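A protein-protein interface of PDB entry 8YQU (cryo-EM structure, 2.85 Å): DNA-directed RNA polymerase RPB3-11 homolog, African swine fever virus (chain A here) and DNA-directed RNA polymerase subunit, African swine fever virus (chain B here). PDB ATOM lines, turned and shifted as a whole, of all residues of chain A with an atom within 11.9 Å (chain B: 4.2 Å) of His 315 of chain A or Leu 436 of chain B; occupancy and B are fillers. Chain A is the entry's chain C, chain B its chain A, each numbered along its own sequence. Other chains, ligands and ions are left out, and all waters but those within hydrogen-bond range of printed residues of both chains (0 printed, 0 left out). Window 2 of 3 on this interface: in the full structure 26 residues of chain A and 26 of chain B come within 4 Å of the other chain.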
ATOM      1  N   ARG A 171     -36.400   2.624   3.741  1.00  0.00           N
ATOM      2  CA  ARG A 171     -34.969   2.365   3.837  1.00  0.00           C
ATOM      3  C   ARG A 171     -34.201   2.894   2.634  1.00  0.00           C
ATOM      4  O   ARG A 171     -33.118   3.461   2.808  1.00  0.00           O
ATOM      5  CB  ARG A 171     -34.707   0.868   3.987  1.00  0.00           C
ATOM      6  CG  ARG A 171     -33.245   0.539   4.219  1.00  0.00           C
ATOM      7  CD  ARG A 171     -33.020  -0.946   4.422  1.00  0.00           C
ATOM      8  NE  ARG A 171     -33.329  -1.730   3.233  1.00  0.00           N
ATOM      9  CZ  ARG A 171     -34.322  -2.605   3.150  1.00  0.00           C
ATOM     10  NH1 ARG A 171     -35.138  -2.823   4.168  1.00  0.00           N
ATOM     11  NH2 ARG A 171     -34.499  -3.280   2.017  1.00  0.00           N
ATOM     12  N   LYS A 172     -34.732   2.719   1.425  1.00  0.00           N
ATOM     13  CA  LYS A 172     -34.054   3.159   0.214  1.00  0.00           C
ATOM     14  C   LYS A 172     -34.014   4.680   0.105  1.00  0.00           C
ATOM     15  O   LYS A 172     -32.970   5.255  -0.216  1.00  0.00           O
ATOM     16  CB  LYS A 172     -34.741   2.554  -1.013  1.00  0.00           C
ATOM     17  CG  LYS A 172     -34.771   1.036  -1.005  1.00  0.00           C
ATOM     18  CD  LYS A 172     -33.369   0.454  -1.008  1.00  0.00           C
ATOM     19  CE  LYS A 172     -33.405  -1.059  -1.124  1.00  0.00           C
ATOM     20  NZ  LYS A 172     -32.048  -1.657  -1.000  1.00  0.00           N
ATOM     21  N   THR A 282     -27.007 -16.681   4.362  1.00  0.00           N
ATOM     22  CA  THR A 282     -26.629 -15.370   3.852  1.00  0.00           C
ATOM     23  C   THR A 282     -27.742 -14.859   2.950  1.00  0.00           C
ATOM     24  O   THR A 282     -28.001 -15.439   1.891  1.00  0.00           O
ATOM     25  CB  THR A 282     -25.307 -15.432   3.087  1.00  0.00           C
ATOM     26  OG1 THR A 282     -24.291 -15.990   3.929  1.00  0.00           O
ATOM     27  CG2 THR A 282     -24.883 -14.042   2.647  1.00  0.00           C
ATOM     28  N   ILE A 283     -28.393 -13.776   3.367  1.00  0.00           N
ATOM     29  CA  ILE A 283     -29.498 -13.189   2.617  1.00  0.00           C
ATOM     30  C   ILE A 283     -29.146 -11.744   2.298  1.00  0.00           C
ATOM     31  O   ILE A 283     -28.737 -10.986   3.186  1.00  0.00           O
ATOM     32  CB  ILE A 283     -30.826 -13.269   3.391  1.00  0.00           C
ATOM     33  CG1 ILE A 283     -31.007 -14.657   4.004  1.00  0.00           C
ATOM     34  CG2 ILE A 283     -31.986 -12.989   2.456  1.00  0.00           C
ATOM     35  CD1 ILE A 283     -31.183 -15.755   2.983  1.00  0.00           C
ATOM     36  N   LYS A 284     -29.308 -11.366   1.035  1.00  0.00           N
ATOM     37  CA  LYS A 284     -28.962 -10.025   0.593  1.00  0.00           C
ATOM     38  C   LYS A 284     -30.105  -9.052   0.854  1.00  0.00           C
ATOM     39  O   LYS A 284     -31.283  -9.423   0.847  1.00  0.00           O
ATOM     40  CB  LYS A 284     -28.607 -10.025  -0.892  1.00  0.00           C
ATOM     41  CG  LYS A 284     -27.313 -10.748  -1.215  1.00  0.00           C
ATOM     42  CD  LYS A 284     -27.054 -10.775  -2.710  1.00  0.00           C
ATOM     43  CE  LYS A 284     -26.695  -9.393  -3.229  1.00  0.00           C
ATOM     44  NZ  LYS A 284     -25.376  -8.932  -2.714  1.00  0.00           N
ATOM     45  N   ASP A 285     -29.737  -7.791   1.089  1.00  0.00           N
ATOM     46  CA  ASP A 285     -30.688  -6.701   1.315  1.00  0.00           C
ATOM     47  C   ASP A 285     -31.608  -6.970   2.502  1.00  0.00           C
ATOM     48  O   ASP A 285     -32.791  -6.624   2.473  1.00  0.00           O
ATOM     49  CB  ASP A 285     -31.512  -6.409   0.056  1.00  0.00           C
ATOM     50  CG  ASP A 285     -30.682  -5.790  -1.052  1.00  0.00           C
ATOM     51  OD1 ASP A 285     -29.694  -5.092  -0.739  1.00  0.00           O
ATOM     52  OD2 ASP A 285     -31.020  -5.996  -2.237  1.00  0.00           O
ATOM     53  N   GLU A 286     -31.079  -7.588   3.552  1.00  0.00           N
ATOM     54  CA  GLU A 286     -31.808  -7.761   4.799  1.00  0.00           C
ATOM     55  C   GLU A 286     -31.230  -6.866   5.885  1.00  0.00           C
ATOM     56  O   GLU A 286     -30.047  -6.518   5.871  1.00  0.00           O
ATOM     57  CB  GLU A 286     -31.786  -9.217   5.262  1.00  0.00           C
ATOM     58  CG  GLU A 286     -32.574 -10.142   4.370  1.00  0.00           C
ATOM     59  CD  GLU A 286     -34.062  -9.851   4.408  1.00  0.00           C
ATOM     60  OE1 GLU A 286     -34.556  -9.415   5.469  1.00  0.00           O
ATOM     61  OE2 GLU A 286     -34.738 -10.056   3.378  1.00  0.00           O
ATOM     62  N   THR A 287     -32.085  -6.502   6.831  1.00  0.00           N
ATOM     63  CA  THR A 287     -31.753  -5.572   7.895  1.00  0.00           C
ATOM     64  C   THR A 287     -31.661  -6.313   9.225  1.00  0.00           C
ATOM     65  O   THR A 287     -31.798  -7.536   9.298  1.00  0.00           O
ATOM     66  CB  THR A 287     -32.788  -4.450   7.964  1.00  0.00           C
ATOM     67  OG1 THR A 287     -34.106  -5.014   7.955  1.00  0.00           O
ATOM     68  CG2 THR A 287     -32.637  -3.527   6.776  1.00  0.00           C
ATOM     69  N   HIS A 288     -31.427  -5.545  10.290  1.00  0.00           N
ATOM     70  CA  HIS A 288     -31.300  -6.131  11.617  1.00  0.00           C
ATOM     71  C   HIS A 288     -32.621  -6.675  12.140  1.00  0.00           C
ATOM     72  O   HIS A 288     -32.617  -7.430  13.116  1.00  0.00           O
ATOM     73  CB  HIS A 288     -30.738  -5.099  12.594  1.00  0.00           C
ATOM     74  CG  HIS A 288     -29.344  -4.660  12.271  1.00  0.00           C
ATOM     75  ND1 HIS A 288     -28.228  -5.288  12.781  1.00  0.00           N
ATOM     76  CD2 HIS A 288     -28.884  -3.657  11.486  1.00  0.00           C
ATOM     77  CE1 HIS A 288     -27.142  -4.691  12.327  1.00  0.00           C
ATOM     78  NE2 HIS A 288     -27.512  -3.698  11.539  1.00  0.00           N
ATOM     79  N   GLN A 311     -25.031 -11.384  11.895  1.00  0.00           N
ATOM     80  CA  GLN A 311     -24.216 -10.237  11.500  1.00  0.00           C
ATOM     81  C   GLN A 311     -24.711  -9.591  10.210  1.00  0.00           C
ATOM     82  O   GLN A 311     -24.659 -10.198   9.138  1.00  0.00           O
ATOM     83  CB  GLN A 311     -22.760 -10.674  11.343  1.00  0.00           C
ATOM     84  CG  GLN A 311     -21.801  -9.542  11.033  1.00  0.00           C
ATOM     85  CD  GLN A 311     -20.433 -10.042  10.623  1.00  0.00           C
ATOM     86  OE1 GLN A 311     -20.249 -11.231  10.362  1.00  0.00           O
ATOM     87  NE2 GLN A 311     -19.463  -9.138  10.566  1.00  0.00           N
ATOM     88  N   CYS A 312     -25.198  -8.357  10.321  1.00  0.00           N
ATOM     89  CA  CYS A 312     -25.602  -7.556   9.171  1.00  0.00           C
ATOM     90  C   CYS A 312     -24.486  -6.564   8.879  1.00  0.00           C
ATOM     91  O   CYS A 312     -24.155  -5.736   9.733  1.00  0.00           O
ATOM     92  CB  CYS A 312     -26.910  -6.812   9.441  1.00  0.00           C
ATOM     93  SG  CYS A 312     -28.310  -7.848   9.888  1.00  0.00           S
ATOM     94  N   VAL A 313     -23.913  -6.639   7.689  1.00  0.00           N
ATOM     95  CA  VAL A 313     -22.716  -5.868   7.352  1.00  0.00           C
ATOM     96  C   VAL A 313     -23.128  -4.663   6.514  1.00  0.00           C
ATOM     97  O   VAL A 313     -23.839  -4.836   5.515  1.00  0.00           O
ATOM     98  CB  VAL A 313     -21.672  -6.720   6.611  1.00  0.00           C
ATOM     99  CG1 VAL A 313     -20.472  -5.865   6.246  1.00  0.00           C
ATOM    100  CG2 VAL A 313     -21.247  -7.896   7.473  1.00  0.00           C
ATOM    101  N   PRO A 314     -22.718  -3.444   6.884  1.00  0.00           N
ATOM    102  CA  PRO A 314     -23.133  -2.255   6.124  1.00  0.00           C
ATOM    103  C   PRO A 314     -22.606  -2.229   4.699  1.00  0.00           C
ATOM    104  O   PRO A 314     -23.368  -1.980   3.761  1.00  0.00           O
ATOM    105  CB  PRO A 314     -22.555  -1.098   6.949  1.00  0.00           C
ATOM    106  CG  PRO A 314     -22.396  -1.655   8.324  1.00  0.00           C
ATOM    107  CD  PRO A 314     -21.995  -3.083   8.113  1.00  0.00           C
ATOM    108  N   HIS A 315     -21.311  -2.485   4.517  1.00  0.00           N
ATOM    109  CA  HIS A 315     -20.704  -2.377   3.196  1.00  0.00           C
ATOM    110  C   HIS A 315     -20.878  -3.632   2.353  1.00  0.00           C
ATOM    111  O   HIS A 315     -20.437  -3.647   1.199  1.00  0.00           O
ATOM    112  CB  HIS A 315     -19.215  -2.038   3.322  1.00  0.00           C
ATOM    113  CG  HIS A 315     -18.388  -3.128   3.927  1.00  0.00           C
ATOM    114  ND1 HIS A 315     -17.870  -4.169   3.187  1.00  0.00           N
ATOM    115  CD2 HIS A 315     -17.977  -3.332   5.202  1.00  0.00           C
ATOM    116  CE1 HIS A 315     -17.181  -4.970   3.980  1.00  0.00           C
ATOM    117  NE2 HIS A 315     -17.230  -4.485   5.207  1.00  0.00           N
ATOM    118  N   LYS A 316     -21.505  -4.678   2.890  1.00  0.00           N
ATOM    119  CA  LYS A 316     -21.836  -5.863   2.115  1.00  0.00           C
ATOM    120  C   LYS A 316     -23.321  -5.977   1.811  1.00  0.00           C
ATOM    121  O   LYS A 316     -23.705  -6.830   1.002  1.00  0.00           O
ATOM    122  CB  LYS A 316     -21.365  -7.130   2.845  1.00  0.00           C
ATOM    123  CG  LYS A 316     -19.857  -7.216   3.018  1.00  0.00           C
ATOM    124  CD  LYS A 316     -19.452  -8.483   3.753  1.00  0.00           C
ATOM    125  CE  LYS A 316     -19.488  -9.693   2.836  1.00  0.00           C
ATOM    126  NZ  LYS A 316     -18.463  -9.605   1.762  1.00  0.00           N
ATOM    127  N   GLN A 317     -24.158  -5.139   2.428  1.00  0.00           N
ATOM    128  CA  GLN A 317     -25.602  -5.119   2.189  1.00  0.00           C
ATOM    129  C   GLN A 317     -26.223  -6.502   2.362  1.00  0.00           C
ATOM    130  O   GLN A 317     -27.065  -6.924   1.568  1.00  0.00           O
ATOM    131  CB  GLN A 317     -25.938  -4.555   0.805  1.00  0.00           C
ATOM    132  CG  GLN A 317     -25.627  -3.077   0.607  1.00  0.00           C
ATOM    133  CD  GLN A 317     -24.183  -2.819   0.235  1.00  0.00           C
ATOM    134  OE1 GLN A 317     -23.467  -3.724  -0.190  1.00  0.00           O
ATOM    135  NE2 GLN A 317     -23.749  -1.574   0.383  1.00  0.00           N
ATOM    136  N   GLU A 318     -25.813  -7.220   3.406  1.00  0.00           N
ATOM    137  CA  GLU A 318     -26.349  -8.559   3.598  1.00  0.00           C
ATOM    138  C   GLU A 318     -26.315  -8.941   5.071  1.00  0.00           C
ATOM    139  O   GLU A 318     -25.539  -8.398   5.870  1.00  0.00           O
ATOM    140  CB  GLU A 318     -25.586  -9.594   2.766  1.00  0.00           C
ATOM    141  CG  GLU A 318     -24.196  -9.908   3.279  1.00  0.00           C
ATOM    142  CD  GLU A 318     -23.418 -10.791   2.326  1.00  0.00           C
ATOM    143  OE1 GLU A 318     -23.919 -11.049   1.213  1.00  0.00           O
ATOM    144  OE2 GLU A 318     -22.310 -11.232   2.695  1.00  0.00           O
ATOM    145  N   MET A 319     -27.166  -9.912   5.399  1.00  0.00           N
ATOM    146  CA  MET A 319     -27.276 -10.495   6.727  1.00  0.00           C
ATOM    147  C   MET A 319     -26.790 -11.935   6.671  1.00  0.00           C
ATOM    148  O   MET A 319     -27.275 -12.728   5.856  1.00  0.00           O
ATOM    149  CB  MET A 319     -28.725 -10.434   7.223  1.00  0.00           C
ATOM    150  CG  MET A 319     -28.970 -10.973   8.629  1.00  0.00           C
ATOM    151  SD  MET A 319     -29.166 -12.762   8.740  1.00  0.00           S
ATOM    152  CE  MET A 319     -30.787 -12.968   8.008  1.00  0.00           C
ATOM    153  N   VAL A 320     -25.840 -12.271   7.540  1.00  0.00           N
ATOM    154  CA  VAL A 320     -25.282 -13.612   7.638  1.00  0.00           C
ATOM    155  C   VAL A 320     -25.622 -14.141   9.022  1.00  0.00           C
ATOM    156  O   VAL A 320     -25.124 -13.627  10.032  1.00  0.00           O
ATOM    157  CB  VAL A 320     -23.766 -13.624   7.399  1.00  0.00           C
ATOM    158  CG1 VAL A 320     -23.241 -15.047   7.406  1.00  0.00           C
ATOM    159  CG2 VAL A 320     -23.429 -12.932   6.091  1.00  0.00           C
ATOM    160  N   ASN B 330     -13.600   2.510   8.707  1.00  0.00           N
ATOM    161  CA  ASN B 330     -14.443   1.332   8.528  1.00  0.00           C
ATOM    162  C   ASN B 330     -13.954   0.266   9.499  1.00  0.00           C
ATOM    163  O   ASN B 330     -12.888  -0.317   9.292  1.00  0.00           O
ATOM    164  CB  ASN B 330     -14.397   0.832   7.088  1.00  0.00           C
ATOM    165  CG  ASN B 330     -15.536  -0.112   6.761  1.00  0.00           C
ATOM    166  OD1 ASN B 330     -16.269  -0.549   7.646  1.00  0.00           O
ATOM    167  ND2 ASN B 330     -15.692  -0.429   5.481  1.00  0.00           N
ATOM    168  N   ASP B 332     -15.230  -2.646  10.113  1.00  0.00           N
ATOM    169  CA  ASP B 332     -15.465  -4.016   9.685  1.00  0.00           C
ATOM    170  C   ASP B 332     -14.365  -4.555   8.782  1.00  0.00           C
ATOM    171  O   ASP B 332     -14.407  -5.735   8.417  1.00  0.00           O
ATOM    172  CB  ASP B 332     -16.812  -4.124   8.966  1.00  0.00           C
ATOM    173  CG  ASP B 332     -17.981  -4.154   9.926  1.00  0.00           C
ATOM    174  OD1 ASP B 332     -17.838  -4.742  11.019  1.00  0.00           O
ATOM    175  OD2 ASP B 332     -19.043  -3.590   9.592  1.00  0.00           O
ATOM    176  N   GLY B 339     -10.852  -0.730   1.914  1.00  0.00           N
ATOM    177  CA  GLY B 339     -12.095  -0.610   1.181  1.00  0.00           C
ATOM    178  C   GLY B 339     -11.896   0.216  -0.070  1.00  0.00           C
ATOM    179  O   GLY B 339     -11.433   1.357   0.006  1.00  0.00           O
ATOM    180  N   TYR B 340     -12.241  -0.342  -1.226  1.00  0.00           N
ATOM    181  CA  TYR B 340     -11.895   0.271  -2.500  1.00  0.00           C
ATOM    182  C   TYR B 340     -13.135   0.324  -3.383  1.00  0.00           C
ATOM    183  O   TYR B 340     -13.769  -0.722  -3.612  1.00  0.00           O
ATOM    184  CB  TYR B 340     -10.769  -0.523  -3.163  1.00  0.00           C
ATOM    185  CG  TYR B 340     -10.243   0.049  -4.454  1.00  0.00           C
ATOM    186  CD1 TYR B 340      -9.435   1.176  -4.450  1.00  0.00           C
ATOM    187  CD2 TYR B 340     -10.501  -0.566  -5.668  1.00  0.00           C
ATOM    188  CE1 TYR B 340      -8.935   1.698  -5.618  1.00  0.00           C
ATOM    189  CE2 TYR B 340      -9.997  -0.052  -6.843  1.00  0.00           C
ATOM    190  CZ  TYR B 340      -9.213   1.079  -6.812  1.00  0.00           C
ATOM    191  OH  TYR B 340      -8.710   1.601  -7.980  1.00  0.00           O
ATOM    192  N   PRO B 341     -13.528   1.496  -3.881  1.00  0.00           N
ATOM    193  CA  PRO B 341     -14.803   1.608  -4.601  1.00  0.00           C
ATOM    194  C   PRO B 341     -14.839   0.751  -5.858  1.00  0.00           C
ATOM    195  O   PRO B 341     -13.821   0.517  -6.512  1.00  0.00           O
ATOM    196  CB  PRO B 341     -14.885   3.099  -4.947  1.00  0.00           C
ATOM    197  CG  PRO B 341     -14.012   3.766  -3.945  1.00  0.00           C
ATOM    198  CD  PRO B 341     -12.894   2.808  -3.677  1.00  0.00           C
ATOM    199  N   ILE B 342     -16.045   0.282  -6.190  1.00  0.00           N
ATOM    200  CA  ILE B 342     -16.227  -0.535  -7.384  1.00  0.00           C
ATOM    201  C   ILE B 342     -15.964   0.278  -8.646  1.00  0.00           C
ATOM    202  O   ILE B 342     -15.452  -0.255  -9.638  1.00  0.00           O
ATOM    203  CB  ILE B 342     -17.635  -1.162  -7.392  1.00  0.00           C
ATOM    204  CG1 ILE B 342     -17.811  -2.077  -8.605  1.00  0.00           C
ATOM    205  CG2 ILE B 342     -18.712  -0.088  -7.353  1.00  0.00           C
ATOM    206  CD1 ILE B 342     -19.015  -2.977  -8.517  1.00  0.00           C
ATOM    207  N   VAL B 434     -10.849  -4.959  -0.636  1.00  0.00           N
ATOM    208  CA  VAL B 434     -12.251  -5.314  -0.459  1.00  0.00           C
ATOM    209  C   VAL B 434     -13.055  -4.327  -1.289  1.00  0.00           C
ATOM    210  O   VAL B 434     -13.112  -3.134  -0.969  1.00  0.00           O
ATOM    211  CB  VAL B 434     -12.671  -5.281   1.016  1.00  0.00           C
ATOM    212  CG1 VAL B 434     -14.181  -5.393   1.138  1.00  0.00           C
ATOM    213  CG2 VAL B 434     -11.991  -6.398   1.781  1.00  0.00           C
ATOM    214  N   VAL B 435     -13.669  -4.813  -2.362  1.00  0.00           N
ATOM    215  CA  VAL B 435     -14.379  -3.939  -3.286  1.00  0.00           C
ATOM    216  C   VAL B 435     -15.757  -3.627  -2.719  1.00  0.00           C
ATOM    217  O   VAL B 435     -16.520  -4.536  -2.373  1.00  0.00           O
ATOM    218  CB  VAL B 435     -14.479  -4.581  -4.677  1.00  0.00           C
ATOM    219  CG1 VAL B 435     -15.491  -3.838  -5.529  1.00  0.00           C
ATOM    220  CG2 VAL B 435     -13.116  -4.586  -5.348  1.00  0.00           C
ATOM    221  N   LEU B 436     -16.073  -2.340  -2.623  1.00  0.00           N
ATOM    222  CA  LEU B 436     -17.343  -1.881  -2.072  1.00  0.00           C
ATOM    223  C   LEU B 436     -18.359  -1.801  -3.206  1.00  0.00           C
ATOM    224  O   LEU B 436     -18.222  -0.975  -4.113  1.00  0.00           O
ATOM    225  CB  LEU B 436     -17.167  -0.531  -1.383  1.00  0.00           C
ATOM    226  CG  LEU B 436     -16.009  -0.461  -0.385  1.00  0.00           C
ATOM    227  CD1 LEU B 436     -15.778   0.965   0.077  1.00  0.00           C
ATOM    228  CD2 LEU B 436     -16.258  -1.376   0.804  1.00  0.00           C
ATOM    229  N   GLU B 437     -19.378  -2.660  -3.152  1.00  0.00           N
ATOM    230  CA  GLU B 437     -20.372  -2.729  -4.215  1.00  0.00           C
ATOM    231  C   GLU B 437     -21.323  -1.541  -4.221  1.00  0.00           C
ATOM    232  O   GLU B 437     -22.060  -1.369  -5.197  1.00  0.00           O
ATOM    233  CB  GLU B 437     -21.173  -4.025  -4.094  1.00  0.00           C
ATOM    234  CG  GLU B 437     -20.323  -5.284  -4.119  1.00  0.00           C
ATOM    235  CD  GLU B 437     -19.929  -5.694  -5.522  1.00  0.00           C
ATOM    236  OE1 GLU B 437     -20.749  -5.517  -6.447  1.00  0.00           O
ATOM    237  OE2 GLU B 437     -18.799  -6.194  -5.701  1.00  0.00           O
ATOM    238  N   ASN B 438     -21.333  -0.732  -3.171  1.00  0.00           N
ATOM    239  CA  ASN B 438     -22.215   0.427  -3.116  1.00  0.00           C
ATOM    240  C   ASN B 438     -21.736   1.484  -4.103  1.00  0.00           C
ATOM    241  O   ASN B 438     -20.596   1.953  -3.986  1.00  0.00           O
ATOM    242  CB  ASN B 438     -22.248   0.988  -1.698  1.00  0.00           C
ATOM    243  CG  ASN B 438     -23.449   1.876  -1.443  1.00  0.00           C
ATOM    244  OD1 ASN B 438     -24.215   2.184  -2.354  1.00  0.00           O
ATOM    245  ND2 ASN B 438     -23.623   2.289  -0.194  1.00  0.00           N
ATOM    246  N   ILE B 441     -20.329   5.121  -2.715  1.00  0.00           N
ATOM    247  CA  ILE B 441     -19.125   5.230  -1.901  1.00  0.00           C
ATOM    248  C   ILE B 441     -17.958   5.590  -2.807  1.00  0.00           C
ATOM    249  O   ILE B 441     -17.685   4.890  -3.791  1.00  0.00           O
ATOM    250  CB  ILE B 441     -18.846   3.923  -1.141  1.00  0.00           C
ATOM    251  CG1 ILE B 441     -20.031   3.564  -0.246  1.00  0.00           C
ATOM    252  CG2 ILE B 441     -17.586   4.060  -0.310  1.00  0.00           C
ATOM    253  CD1 ILE B 441     -20.335   4.598   0.803  1.00  0.00           C
ATOM    254  N   GLN B 445     -11.722   3.219   2.339  1.00  0.00           N
ATOM    255  CA  GLN B 445     -12.020   2.876   3.721  1.00  0.00           C
ATOM    256  C   GLN B 445     -10.992   1.895   4.263  1.00  0.00           C
ATOM    257  O   GLN B 445     -10.582   0.958   3.573  1.00  0.00           O
ATOM    258  CB  GLN B 445     -13.424   2.284   3.836  1.00  0.00           C
ATOM    259  CG  GLN B 445     -14.519   3.231   3.390  1.00  0.00           C
ATOM    260  CD  GLN B 445     -15.895   2.616   3.492  1.00  0.00           C
ATOM    261  OE1 GLN B 445     -16.041   1.457   3.879  1.00  0.00           O
ATOM    262  NE2 GLN B 445     -16.916   3.388   3.145  1.00  0.00           N
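N of Asp 332 of chain B sits close to OD1 of Asn 330 of chain B (3.4 Å).
The backbone NH (N) of Leu 436 of chain B is in hydrogen-bond range of the backbone carbonyl oxygen (O) of Tyr 340 of chain B, at 3.0 Å.
O of Pro 314 of chain A lies within hydrogen-bond range of NE2 of Gln 317 of chain A (3.4 Å).
O of Gln 317 of chain A is in hydrogen-bond range of N of Asp 285 of chain A, at 2.8 Å.
The side-chain amide nitrogen (ND2) of Asn 330 of chain B lies within hydrogen-bond range of the side-chain amide oxygen (OE1) of Gln 445 of chain B (2.5 Å).
O of His 315 of chain A sits close to OE1 of Gln 317 of chain A (3.3 Å).
CD of Pro 314 of chain A touches OD2 of Asp 332 of chain B, at 3.3 Å.
ND2 of Asn 330 of chain B touches CD2 of His 315 of chain A, 3.7 Å away.
Asp 332 of chain B touches His 315 of chain A.
CB of His 315 of chain A touches CD2 of Leu 436 of chain B (3.9 Å).
Asn 438 of chain B touches Gln 317 of chain A (CB to NE2, 3.6 Å).
His 315 of chain A touches three residues of chain B.
Of chain A, only His 315 comes within 4 Å of Leu 436 of chain B.
Asp 332 of chain B touches two residues of chain A.
No residue of chain A comes within 4 Å of Ile 342 of chain B.
Val 434 of chain B touches none of the printed residues of chain A.
No residue of chain A comes within 4 Å of Val 435 of chain B.
Asn 438 of chain B touches just one residue of chain A: Gln 317.
No residue of chain A comes within 4 Å of Ile 441 of chain B.
No residue of chain A comes within 4 Å of Gln 445 of chain B.
Printed residues of chain A within 4 Å of Asn 330 of chain B: His 315.
Of the printed residues of chain B, Pro 314 of chain A touches Asp 332.
Of the printed residues of chain B, Gln 317 of chain A touches Asn 438 (3.6 Å).
Tyr 340 of chain B touches none of the printed residues of chain A.
Of the 19 printed residues of chain A, 3 touch a printed residue of chain B.
Hydrophobic or aromatic side chains of chain A that line the printed part of chain B: Pro 314 and His 315.
Along chain A the printed residues that touch a printed residue of chain B span positions 314 to 317.
Of the 13 printed residues of chain B, 4 touch a printed residue of chain A.
Hydrophobic or aromatic side chains of chain B within 4 Å of the printed part of chain A: Leu 436.
Among the printed residues, 5 pairs touch across the chains.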
